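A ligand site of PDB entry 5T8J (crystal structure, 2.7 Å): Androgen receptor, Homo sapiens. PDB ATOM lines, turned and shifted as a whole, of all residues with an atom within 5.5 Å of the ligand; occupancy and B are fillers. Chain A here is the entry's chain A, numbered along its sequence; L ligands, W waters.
The backbone carbonyl oxygen (O) of Phe 103 lies within hydrogen-bond range of the guanidinium group (NH2) of Arg 91, 3.0 Å away.
The backbone carbonyl oxygen of Leu 40 lies within hydrogen-bond range of the side-chain amide nitrogen of Asn 44, at 3.2 Å.
The indole nitrogen (NE1) of Trp 80 sits at hydrogen-bond distance from the backbone carbonyl oxygen (O) of Gly 47, 3.3 Å away.
SD of Met 84 sits at hydrogen-bond distance from NE1 of Trp 80, 3.3 Å away.
Water W1 lies within hydrogen-bond range of the guanidinium group of Arg 91, the backbone carbonyl oxygen of Met 84, a nitrogen (N2) of the ligand and the side-chain amide nitrogen of Gln 50.
A nitrogen (N2) of the ligand sits close to the backbone carbonyl oxygen of Phe 103, 3.4 Å away.
Merely in contact with the ligand: Leu 40, Leu 43, Asn 44, Leu 46, Gly 47, Met 81, Met 84, Val 85, Met 88, Met 119, Leu 212 and Thr 216.
15 residues have an atom within 4 Å of the ligand: Leu 40, Leu 43, Asn 44, Leu 46, Gly 47, Gln 50, Met 81, Met 84, Val 85, Met 88, Arg 91, Phe 103, Met 119, Leu 212 and Thr 216.
A nitrogen (N2) of the ligand is in hydrogen-bond range of the guanidinium group of Arg 91 (2.9 Å).
A nitrogen (N2) of the ligand sits close to the side-chain amide nitrogen (NE2) of Gln 50 (3.4 Å).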
ATOM      1  N   LEU A  40      21.257  12.405   5.121  1.00  0.00           N
ATOM      2  CA  LEU A  40      20.463  13.535   4.628  1.00  0.00           C
ATOM      3  C   LEU A  40      20.919  14.882   5.168  1.00  0.00           C
ATOM      4  O   LEU A  40      20.676  15.904   4.531  1.00  0.00           O
ATOM      5  CB  LEU A  40      18.977  13.317   4.905  1.00  0.00           C
ATOM      6  CG  LEU A  40      18.210  12.551   3.806  1.00  0.00           C
ATOM      7  CD1 LEU A  40      18.067  13.395   2.538  1.00  0.00           C
ATOM      8  CD2 LEU A  40      18.864  11.198   3.496  1.00  0.00           C
ATOM      9  N   LEU A  43      23.722  15.440   2.590  1.00  0.00           N
ATOM     10  CA  LEU A  43      23.216  15.886   1.273  1.00  0.00           C
ATOM     11  C   LEU A  43      22.763  17.357   1.267  1.00  0.00           C
ATOM     12  O   LEU A  43      22.972  18.076   0.285  1.00  0.00           O
ATOM     13  CB  LEU A  43      22.090  14.969   0.776  1.00  0.00           C
ATOM     14  CG  LEU A  43      22.483  13.609   0.179  1.00  0.00           C
ATOM     15  CD1 LEU A  43      21.201  12.828  -0.044  1.00  0.00           C
ATOM     16  CD2 LEU A  43      23.270  13.685  -1.128  1.00  0.00           C
ATOM     17  N   ASN A  44      22.154  17.806   2.362  1.00  0.00           N
ATOM     18  CA  ASN A  44      21.737  19.213   2.496  1.00  0.00           C
ATOM     19  C   ASN A  44      22.911  20.201   2.580  1.00  0.00           C
ATOM     20  O   ASN A  44      22.794  21.331   2.123  1.00  0.00           O
ATOM     21  CB  ASN A  44      20.795  19.396   3.707  1.00  0.00           C
ATOM     22  CG  ASN A  44      19.452  18.700   3.509  1.00  0.00           C
ATOM     23  OD1 ASN A  44      19.029  18.402   2.381  1.00  0.00           O
ATOM     24  ND2 ASN A  44      18.769  18.447   4.619  1.00  0.00           N
ATOM     25  N   LEU A  46      25.707  19.358   1.015  1.00  0.00           N
ATOM     26  CA  LEU A  46      26.177  19.227  -0.367  1.00  0.00           C
ATOM     27  C   LEU A  46      25.313  20.041  -1.318  1.00  0.00           C
ATOM     28  O   LEU A  46      25.829  20.709  -2.217  1.00  0.00           O
ATOM     29  CB  LEU A  46      26.178  17.766  -0.813  1.00  0.00           C
ATOM     30  CG  LEU A  46      26.687  17.421  -2.233  1.00  0.00           C
ATOM     31  CD1 LEU A  46      28.117  17.899  -2.487  1.00  0.00           C
ATOM     32  CD2 LEU A  46      26.580  15.921  -2.491  1.00  0.00           C
ATOM     33  N   GLY A  47      24.000  19.997  -1.130  1.00  0.00           N
ATOM     34  CA  GLY A  47      23.100  20.820  -1.930  1.00  0.00           C
ATOM     35  C   GLY A  47      23.371  22.315  -1.744  1.00  0.00           C
ATOM     36  O   GLY A  47      23.277  23.081  -2.687  1.00  0.00           O
ATOM     37  N   GLN A  50      26.744  22.911  -3.593  1.00  0.00           N
ATOM     38  CA  GLN A  50      26.472  22.806  -5.020  1.00  0.00           C
ATOM     39  C   GLN A  50      25.747  24.025  -5.562  1.00  0.00           C
ATOM     40  O   GLN A  50      26.008  24.466  -6.684  1.00  0.00           O
ATOM     41  CB  GLN A  50      25.664  21.550  -5.342  1.00  0.00           C
ATOM     42  CG  GLN A  50      26.498  20.266  -5.478  1.00  0.00           C
ATOM     43  CD  GLN A  50      27.495  20.264  -6.653  1.00  0.00           C
ATOM     44  OE1 GLN A  50      27.586  21.240  -7.414  1.00  0.00           O
ATOM     45  NE2 GLN A  50      28.241  19.173  -6.791  1.00  0.00           N
ATOM     46  N   TRP A  80      17.911  24.735  -9.914  1.00  0.00           N
ATOM     47  CA  TRP A  80      19.007  24.212  -9.107  1.00  0.00           C
ATOM     48  C   TRP A  80      19.020  22.695  -8.838  1.00  0.00           C
ATOM     49  O   TRP A  80      20.065  22.067  -8.785  1.00  0.00           O
ATOM     50  CB  TRP A  80      19.059  25.018  -7.793  1.00  0.00           C
ATOM     51  CG  TRP A  80      19.782  24.372  -6.672  1.00  0.00           C
ATOM     52  CD1 TRP A  80      21.137  24.283  -6.499  1.00  0.00           C
ATOM     53  CD2 TRP A  80      19.190  23.736  -5.548  1.00  0.00           C
ATOM     54  NE1 TRP A  80      21.416  23.611  -5.339  1.00  0.00           N
ATOM     55  CE2 TRP A  80      20.243  23.267  -4.723  1.00  0.00           C
ATOM     56  CE3 TRP A  80      17.869  23.515  -5.145  1.00  0.00           C
ATOM     57  CZ2 TRP A  80      20.016  22.582  -3.537  1.00  0.00           C
ATOM     58  CZ3 TRP A  80      17.633  22.827  -3.956  1.00  0.00           C
ATOM     59  CH2 TRP A  80      18.705  22.372  -3.165  1.00  0.00           C
ATOM     60  N   MET A  81      17.849  22.104  -8.659  1.00  0.00           N
ATOM     61  CA  MET A  81      17.747  20.662  -8.341  1.00  0.00           C
ATOM     62  C   MET A  81      18.006  19.765  -9.561  1.00  0.00           C
ATOM     63  O   MET A  81      18.667  18.727  -9.452  1.00  0.00           O
ATOM     64  CB  MET A  81      16.373  20.334  -7.737  1.00  0.00           C
ATOM     65  CG  MET A  81      16.151  18.867  -7.368  1.00  0.00           C
ATOM     66  SD  MET A  81      17.179  18.296  -6.006  1.00  0.00           S
ATOM     67  CE  MET A  81      16.296  18.965  -4.592  1.00  0.00           C
ATOM     68  N   MET A  84      21.778  19.976 -10.531  1.00  0.00           N
ATOM     69  CA  MET A  84      22.589  19.178  -9.597  1.00  0.00           C
ATOM     70  C   MET A  84      22.470  17.712  -9.980  1.00  0.00           C
ATOM     71  O   MET A  84      23.480  17.005 -10.170  1.00  0.00           O
ATOM     72  CB  MET A  84      22.081  19.346  -8.163  1.00  0.00           C
ATOM     73  CG  MET A  84      22.668  20.556  -7.446  1.00  0.00           C
ATOM     74  SD  MET A  84      22.360  20.463  -5.674  1.00  0.00           S
ATOM     75  CE  MET A  84      20.615  20.034  -5.652  1.00  0.00           C
ATOM     76  N   VAL A  85      21.216  17.273 -10.099  1.00  0.00           N
ATOM     77  CA  VAL A  85      20.886  15.932 -10.490  1.00  0.00           C
ATOM     78  C   VAL A  85      21.504  15.566 -11.814  1.00  0.00           C
ATOM     79  O   VAL A  85      21.978  14.440 -11.997  1.00  0.00           O
ATOM     80  CB  VAL A  85      19.372  15.752 -10.622  1.00  0.00           C
ATOM     81  CG1 VAL A  85      19.035  14.467 -11.365  1.00  0.00           C
ATOM     82  CG2 VAL A  85      18.730  15.772  -9.236  1.00  0.00           C
ATOM     83  N   MET A  88      25.317  15.484 -11.313  1.00  0.00           N
ATOM     84  CA  MET A  88      25.512  14.320 -10.455  1.00  0.00           C
ATOM     85  C   MET A  88      25.542  13.068 -11.316  1.00  0.00           C
ATOM     86  O   MET A  88      26.507  12.310 -11.257  1.00  0.00           O
ATOM     87  CB  MET A  88      24.415  14.228  -9.389  1.00  0.00           C
ATOM     88  CG  MET A  88      24.698  13.243  -8.261  1.00  0.00           C
ATOM     89  SD  MET A  88      24.259  11.514  -8.556  1.00  0.00           S
ATOM     90  CE  MET A  88      22.523  11.613  -9.001  1.00  0.00           C
ATOM     91  N   ARG A  91      28.648  12.679 -13.238  1.00  0.00           N
ATOM     92  CA  ARG A  91      29.742  12.232 -12.360  1.00  0.00           C
ATOM     93  C   ARG A  91      29.647  10.724 -12.120  1.00  0.00           C
ATOM     94  O   ARG A  91      30.660  10.013 -12.190  1.00  0.00           O
ATOM     95  CB  ARG A  91      29.700  12.974 -11.020  1.00  0.00           C
ATOM     96  CG  ARG A  91      30.096  14.431 -11.084  1.00  0.00           C
ATOM     97  CD  ARG A  91      30.367  14.964  -9.684  1.00  0.00           C
ATOM     98  NE  ARG A  91      29.158  14.994  -8.858  1.00  0.00           N
ATOM     99  CZ  ARG A  91      28.221  15.943  -8.930  1.00  0.00           C
ATOM    100  NH1 ARG A  91      28.316  16.944  -9.802  1.00  0.00           N
ATOM    101  NH2 ARG A  91      27.170  15.884  -8.125  1.00  0.00           N
ATOM    102  N   PHE A 103      27.386  11.623  -5.769  1.00  0.00           N
ATOM    103  CA  PHE A 103      27.030  12.943  -5.270  1.00  0.00           C
ATOM    104  C   PHE A 103      28.296  13.779  -5.090  1.00  0.00           C
ATOM    105  O   PHE A 103      28.369  14.943  -5.529  1.00  0.00           O
ATOM    106  CB  PHE A 103      26.288  12.829  -3.956  1.00  0.00           C
ATOM    107  CG  PHE A 103      24.974  12.167  -4.096  1.00  0.00           C
ATOM    108  CD1 PHE A 103      23.901  12.874  -4.594  1.00  0.00           C
ATOM    109  CD2 PHE A 103      24.800  10.834  -3.767  1.00  0.00           C
ATOM    110  CE1 PHE A 103      22.662  12.276  -4.746  1.00  0.00           C
ATOM    111  CE2 PHE A 103      23.560  10.231  -3.927  1.00  0.00           C
ATOM    112  CZ  PHE A 103      22.495  10.964  -4.407  1.00  0.00           C
ATOM    113  N   ALA A 104      29.282  13.177  -4.447  1.00  0.00           N
ATOM    114  CA  ALA A 104      30.533  13.835  -4.156  1.00  0.00           C
ATOM    115  C   ALA A 104      31.586  12.764  -4.022  1.00  0.00           C
ATOM    116  O   ALA A 104      31.260  11.585  -3.889  1.00  0.00           O
ATOM    117  CB  ALA A 104      30.424  14.625  -2.851  1.00  0.00           C
ATOM    118  N   MET A 119      15.635   7.271  -0.012  1.00  0.00           N
ATOM    119  CA  MET A 119      15.405   7.865  -1.306  1.00  0.00           C
ATOM    120  C   MET A 119      15.577   6.816  -2.377  1.00  0.00           C
ATOM    121  O   MET A 119      15.966   7.131  -3.517  1.00  0.00           O
ATOM    122  CB  MET A 119      16.412   8.992  -1.561  1.00  0.00           C
ATOM    123  CG  MET A 119      16.167  10.276  -0.780  1.00  0.00           C
ATOM    124  SD  MET A 119      17.463  11.516  -1.040  1.00  0.00           S
ATOM    125  CE  MET A 119      17.794  11.322  -2.793  1.00  0.00           C
ATOM    126  N   MET A 126      17.335   8.618 -10.744  1.00  0.00           N
ATOM    127  CA  MET A 126      18.565   9.369 -10.968  1.00  0.00           C
ATOM    128  C   MET A 126      19.670   8.491 -11.534  1.00  0.00           C
ATOM    129  O   MET A 126      20.489   8.962 -12.321  1.00  0.00           O
ATOM    130  CB  MET A 126      19.060   9.974  -9.659  1.00  0.00           C
ATOM    131  CG  MET A 126      18.199  11.113  -9.149  1.00  0.00           C
ATOM    132  SD  MET A 126      19.011  11.925  -7.766  1.00  0.00           S
ATOM    133  CE  MET A 126      18.533  10.860  -6.402  1.00  0.00           C
ATOM    134  N   LEU A 212      12.302  14.926  -6.244  1.00  0.00           N
ATOM    135  CA  LEU A 212      13.276  15.353  -5.253  1.00  0.00           C
ATOM    136  C   LEU A 212      12.790  16.555  -4.491  1.00  0.00           C
ATOM    137  O   LEU A 212      12.982  16.671  -3.263  1.00  0.00           O
ATOM    138  CB  LEU A 212      14.593  15.680  -5.945  1.00  0.00           C
ATOM    139  CG  LEU A 212      15.283  14.377  -6.348  1.00  0.00           C
ATOM    140  CD1 LEU A 212      16.129  14.557  -7.607  1.00  0.00           C
ATOM    141  CD2 LEU A 212      16.122  13.857  -5.186  1.00  0.00           C
ATOM    142  N   HIS A 213      12.139  17.440  -5.225  1.00  0.00           N
ATOM    143  CA  HIS A 213      11.435  18.553  -4.645  1.00  0.00           C
ATOM    144  C   HIS A 213      10.445  18.076  -3.625  1.00  0.00           C
ATOM    145  O   HIS A 213      10.458  18.510  -2.479  1.00  0.00           O
ATOM    146  CB  HIS A 213      10.701  19.323  -5.712  1.00  0.00           C
ATOM    147  CG  HIS A 213      11.608  20.169  -6.538  1.00  0.00           C
ATOM    148  ND1 HIS A 213      11.737  20.012  -7.892  1.00  0.00           N
ATOM    149  CD2 HIS A 213      12.457  21.168  -6.179  1.00  0.00           C
ATOM    150  CE1 HIS A 213      12.617  20.896  -8.349  1.00  0.00           C
ATOM    151  NE2 HIS A 213      13.064  21.612  -7.327  1.00  0.00           N
ATOM    152  N   PHE A 215      10.158  15.311  -2.040  1.00  0.00           N
ATOM    153  CA  PHE A 215      10.837  14.672  -0.918  1.00  0.00           C
ATOM    154  C   PHE A 215      11.528  15.657   0.019  1.00  0.00           C
ATOM    155  O   PHE A 215      11.409  15.532   1.239  1.00  0.00           O
ATOM    156  CB  PHE A 215      11.896  13.710  -1.463  1.00  0.00           C
ATOM    157  CG  PHE A 215      12.783  13.097  -0.414  1.00  0.00           C
ATOM    158  CD1 PHE A 215      12.439  11.887   0.199  1.00  0.00           C
ATOM    159  CD2 PHE A 215      13.971  13.706  -0.052  1.00  0.00           C
ATOM    160  CE1 PHE A 215      13.266  11.319   1.156  1.00  0.00           C
ATOM    161  CE2 PHE A 215      14.799  13.138   0.905  1.00  0.00           C
ATOM    162  CZ  PHE A 215      14.447  11.949   1.518  1.00  0.00           C
ATOM    163  N   THR A 216      12.273  16.599  -0.554  1.00  0.00           N
ATOM    164  CA  THR A 216      13.029  17.549   0.268  1.00  0.00           C
ATOM    165  C   THR A 216      12.089  18.482   1.019  1.00  0.00           C
ATOM    166  O   THR A 216      12.374  18.888   2.142  1.00  0.00           O
ATOM    167  CB  THR A 216      14.019  18.386  -0.573  1.00  0.00           C
ATOM    168  OG1 THR A 216      15.003  18.989   0.286  1.00  0.00           O
ATOM    169  CG2 THR A 216      13.319  19.468  -1.398  1.00  0.00           C
ATOM    170  N   LEU A 219      10.455  16.481   3.571  1.00  0.00           N
ATOM    171  CA  LEU A 219      11.533  16.280   4.524  1.00  0.00           C
ATOM    172  C   LEU A 219      11.785  17.521   5.386  1.00  0.00           C
ATOM    173  O   LEU A 219      11.971  17.415   6.597  1.00  0.00           O
ATOM    174  CB  LEU A 219      12.811  15.890   3.770  1.00  0.00           C
ATOM    175  CG  LEU A 219      14.056  15.603   4.617  1.00  0.00           C
ATOM    176  CD1 LEU A 219      13.746  14.660   5.782  1.00  0.00           C
ATOM    177  CD2 LEU A 219      15.138  15.043   3.717  1.00  0.00           C
ATOM    178  N   MET A 234      19.113  26.603   1.652  1.00  0.00           N
ATOM    179  CA  MET A 234      18.232  25.463   1.419  1.00  0.00           C
ATOM    180  C   MET A 234      16.817  25.808   1.873  1.00  0.00           C
ATOM    181  O   MET A 234      15.943  26.054   1.036  1.00  0.00           O
ATOM    182  CB  MET A 234      18.751  24.213   2.155  1.00  0.00           C
ATOM    183  CG  MET A 234      19.969  23.568   1.541  1.00  0.00           C
ATOM    184  SD  MET A 234      19.730  23.220  -0.211  1.00  0.00           S
ATOM    185  CE  MET A 234      20.212  24.763  -0.996  1.00  0.00           C
ATOM    186  N   ILE A 238      13.663  25.884  -0.436  1.00  0.00           N
ATOM    187  CA  ILE A 238      12.744  24.772  -0.352  1.00  0.00           C
ATOM    188  C   ILE A 238      11.364  25.211   0.088  1.00  0.00           C
ATOM    189  O   ILE A 238      10.372  24.723  -0.452  1.00  0.00           O
ATOM    190  CB  ILE A 238      13.294  23.687   0.586  1.00  0.00           C
ATOM    191  CG1 ILE A 238      14.512  23.045  -0.066  1.00  0.00           C
ATOM    192  CG2 ILE A 238      12.241  22.621   0.855  1.00  0.00           C
ATOM    193  CD1 ILE A 238      15.481  22.411   0.905  1.00  0.00           C
HETATM  194  C1  LIG L   1      19.867  18.196  -1.572  1.00  0.00           C
HETATM  195  C2  LIG L   1      18.349  18.322  -1.291  1.00  0.00           C
HETATM  196  C3  LIG L   1      17.831  16.868  -1.429  1.00  0.00           C
HETATM  197  C4  LIG L   1      16.359  16.762  -1.834  1.00  0.00           C
HETATM  198  C5  LIG L   1      21.101  16.812  -3.196  1.00  0.00           C
HETATM  199  C6  LIG L   1      23.473  16.877  -4.697  1.00  0.00           C
HETATM  200  C7  LIG L   1      18.672  14.808  -2.526  1.00  0.00           C
HETATM  201  C8  LIG L   1      18.703  16.332  -2.557  1.00  0.00           C
HETATM  202  N1  LIG L   1      20.042  16.871  -2.262  1.00  0.00           N
HETATM  203  O1  LIG L   1      18.050  16.172  -0.200  1.00  0.00           O
HETATM  204  C9  LIG L   1      22.302  17.319  -2.655  1.00  0.00           C
HETATM  205  C10 LIG L   1      23.455  17.354  -3.386  1.00  0.00           C
HETATM  206  C11 LIG L   1      24.741  16.954  -5.359  1.00  0.00           C
HETATM  207  N2  LIG L   1      25.735  17.009  -5.909  1.00  0.00           N
HETATM  208  C12 LIG L   1      22.304  16.355  -5.291  1.00  0.00           C
HETATM  209  F1  LIG L   1      22.330  15.872  -6.576  1.00  0.00           F
HETATM  210  C13 LIG L   1      21.115  16.314  -4.541  1.00  0.00           C
HETATM  211  C14 LIG L   1      19.922  15.743  -5.268  1.00  0.00           C
HETATM  212  O   HOH W   1      25.784  18.185  -8.850  1.00  0.00           O
